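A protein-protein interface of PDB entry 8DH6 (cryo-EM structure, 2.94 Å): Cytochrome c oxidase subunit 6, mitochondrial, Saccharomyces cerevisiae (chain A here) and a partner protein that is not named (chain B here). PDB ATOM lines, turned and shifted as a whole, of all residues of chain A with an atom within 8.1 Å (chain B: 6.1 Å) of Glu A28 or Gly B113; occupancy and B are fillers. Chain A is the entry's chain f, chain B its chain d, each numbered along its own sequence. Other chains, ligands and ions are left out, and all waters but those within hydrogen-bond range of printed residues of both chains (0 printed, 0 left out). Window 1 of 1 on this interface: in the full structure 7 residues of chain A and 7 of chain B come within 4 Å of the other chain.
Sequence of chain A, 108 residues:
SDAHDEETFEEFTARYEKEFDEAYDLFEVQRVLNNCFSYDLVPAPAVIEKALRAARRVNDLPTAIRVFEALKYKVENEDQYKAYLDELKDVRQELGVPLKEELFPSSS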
ATOM      1  N   GLU A  19     -11.502 -13.455 -15.973  1.00  0.00           N
ATOM      2  CA  GLU A  19     -12.270 -13.920 -14.823  1.00  0.00           C
ATOM      3  C   GLU A  19     -13.145 -15.115 -15.184  1.00  0.00           C
ATOM      4  O   GLU A  19     -13.437 -15.961 -14.332  1.00  0.00           O
ATOM      5  CB  GLU A  19     -13.111 -12.771 -14.270  1.00  0.00           C
ATOM      6  CG  GLU A  19     -13.521 -12.938 -12.824  1.00  0.00           C
ATOM      7  CD  GLU A  19     -14.193 -11.700 -12.275  1.00  0.00           C
ATOM      8  OE1 GLU A  19     -14.984 -11.823 -11.318  1.00  0.00           O
ATOM      9  OE2 GLU A  19     -13.926 -10.602 -12.803  1.00  0.00           O
ATOM     10  N   PHE A  20     -13.579 -15.203 -16.444  1.00  0.00           N
ATOM     11  CA  PHE A  20     -14.234 -16.416 -16.909  1.00  0.00           C
ATOM     12  C   PHE A  20     -13.247 -17.555 -17.116  1.00  0.00           C
ATOM     13  O   PHE A  20     -13.626 -18.720 -16.963  1.00  0.00           O
ATOM     14  CB  PHE A  20     -14.995 -16.151 -18.207  1.00  0.00           C
ATOM     15  CG  PHE A  20     -16.413 -15.710 -17.996  1.00  0.00           C
ATOM     16  CD1 PHE A  20     -17.318 -16.536 -17.359  1.00  0.00           C
ATOM     17  CD2 PHE A  20     -16.844 -14.477 -18.448  1.00  0.00           C
ATOM     18  CE1 PHE A  20     -18.621 -16.137 -17.165  1.00  0.00           C
ATOM     19  CE2 PHE A  20     -18.148 -14.073 -18.258  1.00  0.00           C
ATOM     20  CZ  PHE A  20     -19.037 -14.904 -17.617  1.00  0.00           C
ATOM     21  N   GLU A  22     -10.487 -18.222 -15.260  1.00  0.00           N
ATOM     22  CA  GLU A  22     -10.186 -18.843 -13.971  1.00  0.00           C
ATOM     23  C   GLU A  22     -11.417 -19.268 -13.178  1.00  0.00           C
ATOM     24  O   GLU A  22     -11.266 -19.707 -12.034  1.00  0.00           O
ATOM     25  CB  GLU A  22      -9.300 -17.951 -13.084  1.00  0.00           C
ATOM     26  CG  GLU A  22      -7.834 -17.823 -13.517  1.00  0.00           C
ATOM     27  CD  GLU A  22      -7.582 -16.748 -14.535  1.00  0.00           C
ATOM     28  OE1 GLU A  22      -8.527 -16.017 -14.862  1.00  0.00           O
ATOM     29  OE2 GLU A  22      -6.434 -16.634 -15.009  1.00  0.00           O
ATOM     30  N   ALA A  23     -12.618 -19.152 -13.734  1.00  0.00           N
ATOM     31  CA  ALA A  23     -13.780 -19.752 -13.089  1.00  0.00           C
ATOM     32  C   ALA A  23     -13.622 -21.268 -13.053  1.00  0.00           C
ATOM     33  O   ALA A  23     -13.249 -21.889 -14.052  1.00  0.00           O
ATOM     34  CB  ALA A  23     -15.060 -19.369 -13.827  1.00  0.00           C
ATOM     35  N   TYR A  24     -13.906 -21.870 -11.895  1.00  0.00           N
ATOM     36  CA  TYR A  24     -13.615 -23.284 -11.697  1.00  0.00           C
ATOM     37  C   TYR A  24     -14.825 -24.164 -11.422  1.00  0.00           C
ATOM     38  O   TYR A  24     -14.713 -25.383 -11.576  1.00  0.00           O
ATOM     39  CB  TYR A  24     -12.604 -23.477 -10.552  1.00  0.00           C
ATOM     40  CG  TYR A  24     -12.919 -22.726  -9.278  1.00  0.00           C
ATOM     41  CD1 TYR A  24     -13.727 -23.287  -8.300  1.00  0.00           C
ATOM     42  CD2 TYR A  24     -12.387 -21.466  -9.044  1.00  0.00           C
ATOM     43  CE1 TYR A  24     -14.009 -22.608  -7.132  1.00  0.00           C
ATOM     44  CE2 TYR A  24     -12.664 -20.780  -7.881  1.00  0.00           C
ATOM     45  CZ  TYR A  24     -13.473 -21.354  -6.928  1.00  0.00           C
ATOM     46  OH  TYR A  24     -13.750 -20.670  -5.768  1.00  0.00           O
ATOM     47  N   ASP A  25     -15.966 -23.603 -11.028  1.00  0.00           N
ATOM     48  CA  ASP A  25     -17.155 -24.411 -10.796  1.00  0.00           C
ATOM     49  C   ASP A  25     -18.387 -23.612 -11.199  1.00  0.00           C
ATOM     50  O   ASP A  25     -18.292 -22.462 -11.633  1.00  0.00           O
ATOM     51  CB  ASP A  25     -17.239 -24.877  -9.338  1.00  0.00           C
ATOM     52  CG  ASP A  25     -17.468 -23.735  -8.373  1.00  0.00           C
ATOM     53  OD1 ASP A  25     -17.032 -22.605  -8.670  1.00  0.00           O
ATOM     54  OD2 ASP A  25     -18.083 -23.971  -7.315  1.00  0.00           O
ATOM     55  N   LEU A  26     -19.554 -24.244 -11.053  1.00  0.00           N
ATOM     56  CA  LEU A  26     -20.803 -23.619 -11.474  1.00  0.00           C
ATOM     57  C   LEU A  26     -21.104 -22.354 -10.683  1.00  0.00           C
ATOM     58  O   LEU A  26     -21.564 -21.361 -11.260  1.00  0.00           O
ATOM     59  CB  LEU A  26     -21.955 -24.611 -11.342  1.00  0.00           C
ATOM     60  CG  LEU A  26     -23.330 -24.077 -11.735  1.00  0.00           C
ATOM     61  CD1 LEU A  26     -23.291 -23.553 -13.156  1.00  0.00           C
ATOM     62  CD2 LEU A  26     -24.381 -25.159 -11.585  1.00  0.00           C
ATOM     63  N   PHE A  27     -20.863 -22.370  -9.371  1.00  0.00           N
ATOM     64  CA  PHE A  27     -21.077 -21.172  -8.564  1.00  0.00           C
ATOM     65  C   PHE A  27     -20.250 -20.007  -9.087  1.00  0.00           C
ATOM     66  O   PHE A  27     -20.766 -18.896  -9.248  1.00  0.00           O
ATOM     67  CB  PHE A  27     -20.736 -21.460  -7.102  1.00  0.00           C
ATOM     68  CG  PHE A  27     -21.100 -20.347  -6.156  1.00  0.00           C
ATOM     69  CD1 PHE A  27     -20.253 -19.269  -5.969  1.00  0.00           C
ATOM     70  CD2 PHE A  27     -22.276 -20.395  -5.434  1.00  0.00           C
ATOM     71  CE1 PHE A  27     -20.583 -18.254  -5.100  1.00  0.00           C
ATOM     72  CE2 PHE A  27     -22.610 -19.382  -4.561  1.00  0.00           C
ATOM     73  CZ  PHE A  27     -21.762 -18.311  -4.393  1.00  0.00           C
ATOM     74  N   GLU A  28     -18.967 -20.242  -9.367  1.00  0.00           N
ATOM     75  CA  GLU A  28     -18.107 -19.176  -9.865  1.00  0.00           C
ATOM     76  C   GLU A  28     -18.534 -18.702 -11.247  1.00  0.00           C
ATOM     77  O   GLU A  28     -18.518 -17.497 -11.519  1.00  0.00           O
ATOM     78  CB  GLU A  28     -16.652 -19.638  -9.887  1.00  0.00           C
ATOM     79  CG  GLU A  28     -15.968 -19.544  -8.540  1.00  0.00           C
ATOM     80  CD  GLU A  28     -15.965 -18.134  -7.989  1.00  0.00           C
ATOM     81  OE1 GLU A  28     -15.670 -17.196  -8.756  1.00  0.00           O
ATOM     82  OE2 GLU A  28     -16.263 -17.965  -6.788  1.00  0.00           O
ATOM     83  N   VAL A  29     -18.910 -19.627 -12.132  1.00  0.00           N
ATOM     84  CA  VAL A  29     -19.353 -19.236 -13.467  1.00  0.00           C
ATOM     85  C   VAL A  29     -20.587 -18.350 -13.377  1.00  0.00           C
ATOM     86  O   VAL A  29     -20.662 -17.296 -14.020  1.00  0.00           O
ATOM     87  CB  VAL A  29     -19.617 -20.484 -14.330  1.00  0.00           C
ATOM     88  CG1 VAL A  29     -20.325 -20.098 -15.613  1.00  0.00           C
ATOM     89  CG2 VAL A  29     -18.316 -21.198 -14.638  1.00  0.00           C
ATOM     90  N   GLN A  30     -21.562 -18.753 -12.561  1.00  0.00           N
ATOM     91  CA  GLN A  30     -22.784 -17.970 -12.425  1.00  0.00           C
ATOM     92  C   GLN A  30     -22.512 -16.621 -11.772  1.00  0.00           C
ATOM     93  O   GLN A  30     -23.092 -15.609 -12.174  1.00  0.00           O
ATOM     94  CB  GLN A  30     -23.822 -18.761 -11.632  1.00  0.00           C
ATOM     95  CG  GLN A  30     -24.293 -20.011 -12.350  1.00  0.00           C
ATOM     96  CD  GLN A  30     -25.649 -20.481 -11.882  1.00  0.00           C
ATOM     97  OE1 GLN A  30     -26.000 -20.329 -10.716  1.00  0.00           O
ATOM     98  NE2 GLN A  30     -26.418 -21.062 -12.792  1.00  0.00           N
ATOM     99  N   ARG A  31     -21.629 -16.581 -10.770  1.00  0.00           N
ATOM    100  CA  ARG A  31     -21.306 -15.315 -10.116  1.00  0.00           C
ATOM    101  C   ARG A  31     -20.612 -14.356 -11.077  1.00  0.00           C
ATOM    102  O   ARG A  31     -20.930 -13.159 -11.121  1.00  0.00           O
ATOM    103  CB  ARG A  31     -20.428 -15.573  -8.893  1.00  0.00           C
ATOM    104  CG  ARG A  31     -19.903 -14.312  -8.241  1.00  0.00           C
ATOM    105  CD  ARG A  31     -18.777 -14.609  -7.271  1.00  0.00           C
ATOM    106  NE  ARG A  31     -17.574 -15.066  -7.953  1.00  0.00           N
ATOM    107  CZ  ARG A  31     -16.687 -14.262  -8.523  1.00  0.00           C
ATOM    108  NH1 ARG A  31     -16.851 -12.952  -8.536  1.00  0.00           N
ATOM    109  NH2 ARG A  31     -15.611 -14.789  -9.099  1.00  0.00           N
ATOM    110  N   VAL A  32     -19.648 -14.865 -11.844  1.00  0.00           N
ATOM    111  CA  VAL A  32     -18.936 -14.031 -12.805  1.00  0.00           C
ATOM    112  C   VAL A  32     -19.892 -13.524 -13.875  1.00  0.00           C
ATOM    113  O   VAL A  32     -19.847 -12.353 -14.259  1.00  0.00           O
ATOM    114  CB  VAL A  32     -17.757 -14.809 -13.414  1.00  0.00           C
ATOM    115  CG1 VAL A  32     -17.204 -14.076 -14.616  1.00  0.00           C
ATOM    116  CG2 VAL A  32     -16.673 -15.020 -12.379  1.00  0.00           C
ATOM    117  N   LEU A  33     -20.782 -14.390 -14.362  1.00  0.00           N
ATOM    118  CA  LEU A  33     -21.757 -13.958 -15.355  1.00  0.00           C
ATOM    119  C   LEU A  33     -22.701 -12.906 -14.779  1.00  0.00           C
ATOM    120  O   LEU A  33     -23.030 -11.920 -15.453  1.00  0.00           O
ATOM    121  CB  LEU A  33     -22.525 -15.173 -15.868  1.00  0.00           C
ATOM    122  CG  LEU A  33     -23.627 -14.990 -16.903  1.00  0.00           C
ATOM    123  CD1 LEU A  33     -23.018 -14.596 -18.227  1.00  0.00           C
ATOM    124  CD2 LEU A  33     -24.401 -16.282 -17.041  1.00  0.00           C
ATOM    125  N   ASN A  34     -23.120 -13.086 -13.523  1.00  0.00           N
ATOM    126  CA  ASN A  34     -24.021 -12.134 -12.883  1.00  0.00           C
ATOM    127  C   ASN A  34     -23.381 -10.762 -12.758  1.00  0.00           C
ATOM    128  O   ASN A  34     -23.961  -9.756 -13.183  1.00  0.00           O
ATOM    129  CB  ASN A  34     -24.428 -12.646 -11.504  1.00  0.00           C
ATOM    130  CG  ASN A  34     -25.565 -11.854 -10.906  1.00  0.00           C
ATOM    131  OD1 ASN A  34     -26.420 -11.339 -11.625  1.00  0.00           O
ATOM    132  ND2 ASN A  34     -25.586 -11.755  -9.585  1.00  0.00           N
ATOM    133  N   ASN A  35     -22.185 -10.695 -12.182  1.00  0.00           N
ATOM    134  CA  ASN A  35     -21.566  -9.391 -11.997  1.00  0.00           C
ATOM    135  C   ASN A  35     -20.952  -8.849 -13.281  1.00  0.00           C
ATOM    136  O   ASN A  35     -20.559  -7.681 -13.316  1.00  0.00           O
ATOM    137  CB  ASN A  35     -20.539  -9.432 -10.855  1.00  0.00           C
ATOM    138  CG  ASN A  35     -19.367 -10.349 -11.129  1.00  0.00           C
ATOM    139  OD1 ASN A  35     -19.177 -10.831 -12.240  1.00  0.00           O
ATOM    140  ND2 ASN A  35     -18.569 -10.595 -10.099  1.00  0.00           N
ATOM    141  N   ALA A  54     -17.114 -21.439 -20.382  1.00  0.00           N
ATOM    142  CA  ALA A  54     -17.168 -21.794 -18.967  1.00  0.00           C
ATOM    143  C   ALA A  54     -18.384 -22.653 -18.645  1.00  0.00           C
ATOM    144  O   ALA A  54     -18.285 -23.588 -17.842  1.00  0.00           O
ATOM    145  CB  ALA A  54     -17.171 -20.534 -18.108  1.00  0.00           C
ATOM    146  N   ARG A  57     -17.598 -26.010 -19.765  1.00  0.00           N
ATOM    147  CA  ARG A  57     -16.530 -26.599 -18.963  1.00  0.00           C
ATOM    148  C   ARG A  57     -17.052 -27.177 -17.655  1.00  0.00           C
ATOM    149  O   ARG A  57     -16.543 -28.200 -17.185  1.00  0.00           O
ATOM    150  CB  ARG A  57     -15.451 -25.551 -18.691  1.00  0.00           C
ATOM    151  CG  ARG A  57     -14.298 -26.036 -17.833  1.00  0.00           C
ATOM    152  CD  ARG A  57     -12.985 -25.387 -18.255  1.00  0.00           C
ATOM    153  NE  ARG A  57     -13.081 -23.941 -18.435  1.00  0.00           N
ATOM    154  CZ  ARG A  57     -13.430 -23.073 -17.494  1.00  0.00           C
ATOM    155  NH1 ARG A  57     -13.679 -23.456 -16.252  1.00  0.00           N
ATOM    156  NH2 ARG A  57     -13.515 -21.783 -17.804  1.00  0.00           N
ATOM    157  N   VAL A  58     -18.054 -26.540 -17.048  1.00  0.00           N
ATOM    158  CA  VAL A  58     -18.645 -27.025 -15.808  1.00  0.00           C
ATOM    159  C   VAL A  58     -19.870 -27.895 -16.066  1.00  0.00           C
ATOM    160  O   VAL A  58     -20.525 -28.333 -15.116  1.00  0.00           O
ATOM    161  CB  VAL A  58     -18.991 -25.861 -14.867  1.00  0.00           C
ATOM    162  CG1 VAL A  58     -17.774 -24.981 -14.649  1.00  0.00           C
ATOM    163  CG2 VAL A  58     -20.142 -25.052 -15.430  1.00  0.00           C
ATOM    164  N   LYS B  66      -8.026 -13.903  -1.922  1.00  0.00           N
ATOM    165  CA  LYS B  66      -9.393 -14.185  -2.344  1.00  0.00           C
ATOM    166  C   LYS B  66     -10.002 -15.373  -1.615  1.00  0.00           C
ATOM    167  O   LYS B  66     -11.195 -15.354  -1.302  1.00  0.00           O
ATOM    168  CB  LYS B  66      -9.446 -14.427  -3.855  1.00  0.00           C
ATOM    169  CG  LYS B  66     -10.856 -14.431  -4.428  1.00  0.00           C
ATOM    170  CD  LYS B  66     -10.978 -15.413  -5.579  1.00  0.00           C
ATOM    171  CE  LYS B  66     -12.323 -15.298  -6.267  1.00  0.00           C
ATOM    172  NZ  LYS B  66     -12.442 -16.254  -7.400  1.00  0.00           N
ATOM    173  N   GLY B  67      -9.223 -16.410  -1.336  1.00  0.00           N
ATOM    174  CA  GLY B  67      -9.760 -17.547  -0.615  1.00  0.00           C
ATOM    175  C   GLY B  67     -10.589 -18.477  -1.473  1.00  0.00           C
ATOM    176  O   GLY B  67     -11.801 -18.593  -1.280  1.00  0.00           O
ATOM    177  N   THR B  68      -9.947 -19.135  -2.435  1.00  0.00           N
ATOM    178  CA  THR B  68     -10.638 -20.049  -3.330  1.00  0.00           C
ATOM    179  C   THR B  68     -11.144 -21.271  -2.563  1.00  0.00           C
ATOM    180  O   THR B  68     -10.890 -21.444  -1.369  1.00  0.00           O
ATOM    181  CB  THR B  68      -9.717 -20.468  -4.471  1.00  0.00           C
ATOM    182  OG1 THR B  68      -8.569 -21.138  -3.936  1.00  0.00           O
ATOM    183  CG2 THR B  68      -9.258 -19.251  -5.254  1.00  0.00           C
ATOM    184  N   MET B  69     -11.872 -22.136  -3.270  1.00  0.00           N
ATOM    185  CA  MET B  69     -12.479 -23.300  -2.635  1.00  0.00           C
ATOM    186  C   MET B  69     -11.450 -24.322  -2.171  1.00  0.00           C
ATOM    187  O   MET B  69     -11.673 -24.984  -1.153  1.00  0.00           O
ATOM    188  CB  MET B  69     -13.470 -23.961  -3.594  1.00  0.00           C
ATOM    189  CG  MET B  69     -14.447 -24.904  -2.920  1.00  0.00           C
ATOM    190  SD  MET B  69     -15.738 -24.028  -2.023  1.00  0.00           S
ATOM    191  CE  MET B  69     -16.787 -25.391  -1.539  1.00  0.00           C
ATOM    192  N   ARG B 108     -19.670 -18.617   0.808  1.00  0.00           N
ATOM    193  CA  ARG B 108     -19.185 -17.970  -0.402  1.00  0.00           C
ATOM    194  C   ARG B 108     -19.911 -16.645  -0.605  1.00  0.00           C
ATOM    195  O   ARG B 108     -21.125 -16.555  -0.404  1.00  0.00           O
ATOM    196  CB  ARG B 108     -19.377 -18.882  -1.612  1.00  0.00           C
ATOM    197  CG  ARG B 108     -19.062 -20.341  -1.329  1.00  0.00           C
ATOM    198  CD  ARG B 108     -19.273 -21.198  -2.561  1.00  0.00           C
ATOM    199  NE  ARG B 108     -18.337 -20.869  -3.627  1.00  0.00           N
ATOM    200  CZ  ARG B 108     -17.783 -21.760  -4.438  1.00  0.00           C
ATOM    201  NH1 ARG B 108     -18.057 -23.049  -4.338  1.00  0.00           N
ATOM    202  NH2 ARG B 108     -16.939 -21.345  -5.378  1.00  0.00           N
ATOM    203  N   CYS B 109     -19.158 -15.618  -1.007  1.00  0.00           N
ATOM    204  CA  CYS B 109     -19.684 -14.256  -1.015  1.00  0.00           C
ATOM    205  C   CYS B 109     -20.773 -14.048  -2.062  1.00  0.00           C
ATOM    206  O   CYS B 109     -21.713 -13.279  -1.826  1.00  0.00           O
ATOM    207  CB  CYS B 109     -18.556 -13.254  -1.242  1.00  0.00           C
ATOM    208  SG  CYS B 109     -19.149 -11.572  -1.534  1.00  0.00           S
ATOM    209  N   TRP B 110     -20.643 -14.694  -3.223  1.00  0.00           N
ATOM    210  CA  TRP B 110     -21.527 -14.528  -4.377  1.00  0.00           C
ATOM    211  C   TRP B 110     -21.268 -13.199  -5.083  1.00  0.00           C
ATOM    212  O   TRP B 110     -21.840 -12.934  -6.147  1.00  0.00           O
ATOM    213  CB  TRP B 110     -23.006 -14.660  -3.979  1.00  0.00           C
ATOM    214  CG  TRP B 110     -23.964 -14.344  -5.084  1.00  0.00           C
ATOM    215  CD1 TRP B 110     -24.736 -13.226  -5.206  1.00  0.00           C
ATOM    216  CD2 TRP B 110     -24.226 -15.138  -6.247  1.00  0.00           C
ATOM    217  NE1 TRP B 110     -25.473 -13.284  -6.362  1.00  0.00           N
ATOM    218  CE2 TRP B 110     -25.176 -14.447  -7.020  1.00  0.00           C
ATOM    219  CE3 TRP B 110     -23.753 -16.371  -6.703  1.00  0.00           C
ATOM    220  CZ2 TRP B 110     -25.662 -14.947  -8.222  1.00  0.00           C
ATOM    221  CZ3 TRP B 110     -24.237 -16.864  -7.897  1.00  0.00           C
ATOM    222  CH2 TRP B 110     -25.181 -16.155  -8.643  1.00  0.00           C
ATOM    223  N   GLU B 111     -20.390 -12.363  -4.535  1.00  0.00           N
ATOM    224  CA  GLU B 111     -19.992 -11.140  -5.219  1.00  0.00           C
ATOM    225  C   GLU B 111     -18.498 -11.082  -5.497  1.00  0.00           C
ATOM    226  O   GLU B 111     -18.090 -10.644  -6.576  1.00  0.00           O
ATOM    227  CB  GLU B 111     -20.427  -9.909  -4.416  1.00  0.00           C
ATOM    228  CG  GLU B 111     -20.267  -8.609  -5.179  1.00  0.00           C
ATOM    229  CD  GLU B 111     -20.896  -7.435  -4.466  1.00  0.00           C
ATOM    230  OE1 GLU B 111     -21.418  -7.627  -3.349  1.00  0.00           O
ATOM    231  OE2 GLU B 111     -20.876  -6.320  -5.027  1.00  0.00           O
ATOM    232  N   CYS B 112     -17.662 -11.510  -4.551  1.00  0.00           N
ATOM    233  CA  CYS B 112     -16.234 -11.641  -4.799  1.00  0.00           C
ATOM    234  C   CYS B 112     -15.768 -13.088  -4.826  1.00  0.00           C
ATOM    235  O   CYS B 112     -14.621 -13.342  -5.204  1.00  0.00           O
ATOM    236  CB  CYS B 112     -15.423 -10.860  -3.752  1.00  0.00           C
ATOM    237  SG  CYS B 112     -15.472 -11.500  -2.064  1.00  0.00           S
ATOM    238  N   GLY B 113     -16.622 -14.036  -4.447  1.00  0.00           N
ATOM    239  CA  GLY B 113     -16.294 -15.442  -4.540  1.00  0.00           C
ATOM    240  C   GLY B 113     -15.459 -15.998  -3.412  1.00  0.00           C
ATOM    241  O   GLY B 113     -15.065 -17.168  -3.480  1.00  0.00           O
ATOM    242  N   SER B 114     -15.173 -15.208  -2.381  1.00  0.00           N
ATOM    243  CA  SER B 114     -14.347 -15.683  -1.282  1.00  0.00           C
ATOM    244  C   SER B 114     -15.039 -16.814  -0.533  1.00  0.00           C
ATOM    245  O   SER B 114     -16.246 -16.774  -0.289  1.00  0.00           O
ATOM    246  CB  SER B 114     -14.030 -14.543  -0.318  1.00  0.00           C
ATOM    247  OG  SER B 114     -13.458 -13.443  -1.001  1.00  0.00           O
ATOM    248  N   VAL B 115     -14.258 -17.826  -0.166  1.00  0.00           N
ATOM    249  CA  VAL B 115     -14.751 -18.985   0.569  1.00  0.00           C
ATOM    250  C   VAL B 115     -14.151 -18.935   1.964  1.00  0.00           C
ATOM    251  O   VAL B 115     -12.926 -18.852   2.116  1.00  0.00           O
ATOM    252  CB  VAL B 115     -14.395 -20.303  -0.133  1.00  0.00           C
ATOM    253  CG1 VAL B 115     -14.829 -21.483   0.708  1.00  0.00           C
ATOM    254  CG2 VAL B 115     -15.039 -20.358  -1.502  1.00  0.00           C
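The side-chain amide oxygen (OD1) of Asn A35 lies close to the backbone carbonyl oxygen (O) of Val A32, at 2.6 Å.
OE1 of Glu A19 is in salt-bridge range of NH1 of Arg A31 (3.5 Å).
The guanidinium group of Arg B108 lies within hydrogen-bond range of the side-chain sulfur of Met B69 (3.4 Å).
The backbone carbonyl oxygen (O) of Arg A31 sits close to the side-chain amide oxygen (OD1) of Asn A35, 3.1 Å away.
The side-chain sulfur of Cys B109 lies close to the backbone NH of Glu B111, at 3.3 Å.
The side-chain carboxylate (OD1) of Asp A25 is in hydrogen-bond range of the backbone NH (N) of Glu A28 (3.1 Å).
NH2 of Arg B108 sits at hydrogen-bond distance from OH of Tyr A24.
The backbone NH (N) of Met B69 lies within hydrogen-bond range of the side-chain hydroxyl (OH) of Tyr A24 (3.5 Å).
The side-chain carboxylate of Glu A28 is in salt-bridge range of the side-chain amino group of Lys B66 (3.6 Å).
NH2 of Arg B108 is in salt-bridge range of OE2 of Glu A28, at 3.7 Å.
The guanidinium group (NH1) of Arg B108 lies within salt-bridge range of the side-chain carboxylate (OD2) of Asp A25 (3.1 Å).
The backbone carbonyl oxygen of Glu B111 lies within hydrogen-bond range of the guanidinium group of Arg A31.
Among the printed residues, pairs that only touch across the chains: Phe A27 with Arg B108 (3.4 Å), Phe A27 with Trp B110 (3.6 Å), Glu A28 with Gly B113 (3.4 Å), Arg A31 with Lys B66 (3.9 Å), Arg A31 with Trp B110 (3.2 Å), Arg A31 with Cys B112 (3.9 Å), Arg A31 with Gly B113 (3.6 Å), Asn A34 with Trp B110 (3.5 Å) and Asn A35 with Glu B111 (3.6 Å).
Hydrophobic or aromatic side chains of chain B within 4 Å of the printed part of chain A: Met B69 and Trp B110.
Of the 19 printed residues of chain A, 7 touch a printed residue of chain B.
Hydrophobic or aromatic side chains of chain A within 4 Å of the printed part of chain B: Tyr A24 and Phe A27.
Among the printed residues, 15 pairs touch across the chains.
Of chain B, only Lys B66 (3.6 Å), Arg B108 (3.7 Å) and Gly B113 (3.4 Å) come within 4 Å of Glu A28.
Val A29 touches none of the printed residues of chain B.
Of the printed residues of chain B, Asn A35 touches Glu B111 (3.6 Å).
Of the printed residues of chain A, Lys B66 touches Glu A28 (3.6 Å) and Arg A31 (3.9 Å).
Of chain A, only Arg A31 comes within 4 Å of Cys B112.
Ser B114 touches none of the printed residues of chain A.
The nearest residue of chain B that does not touch Glu A28 is Cys B112 (5.2 Å).
The nearest residue of chain A that does not touch Gly B113 is Tyr A24 (4.4 Å).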
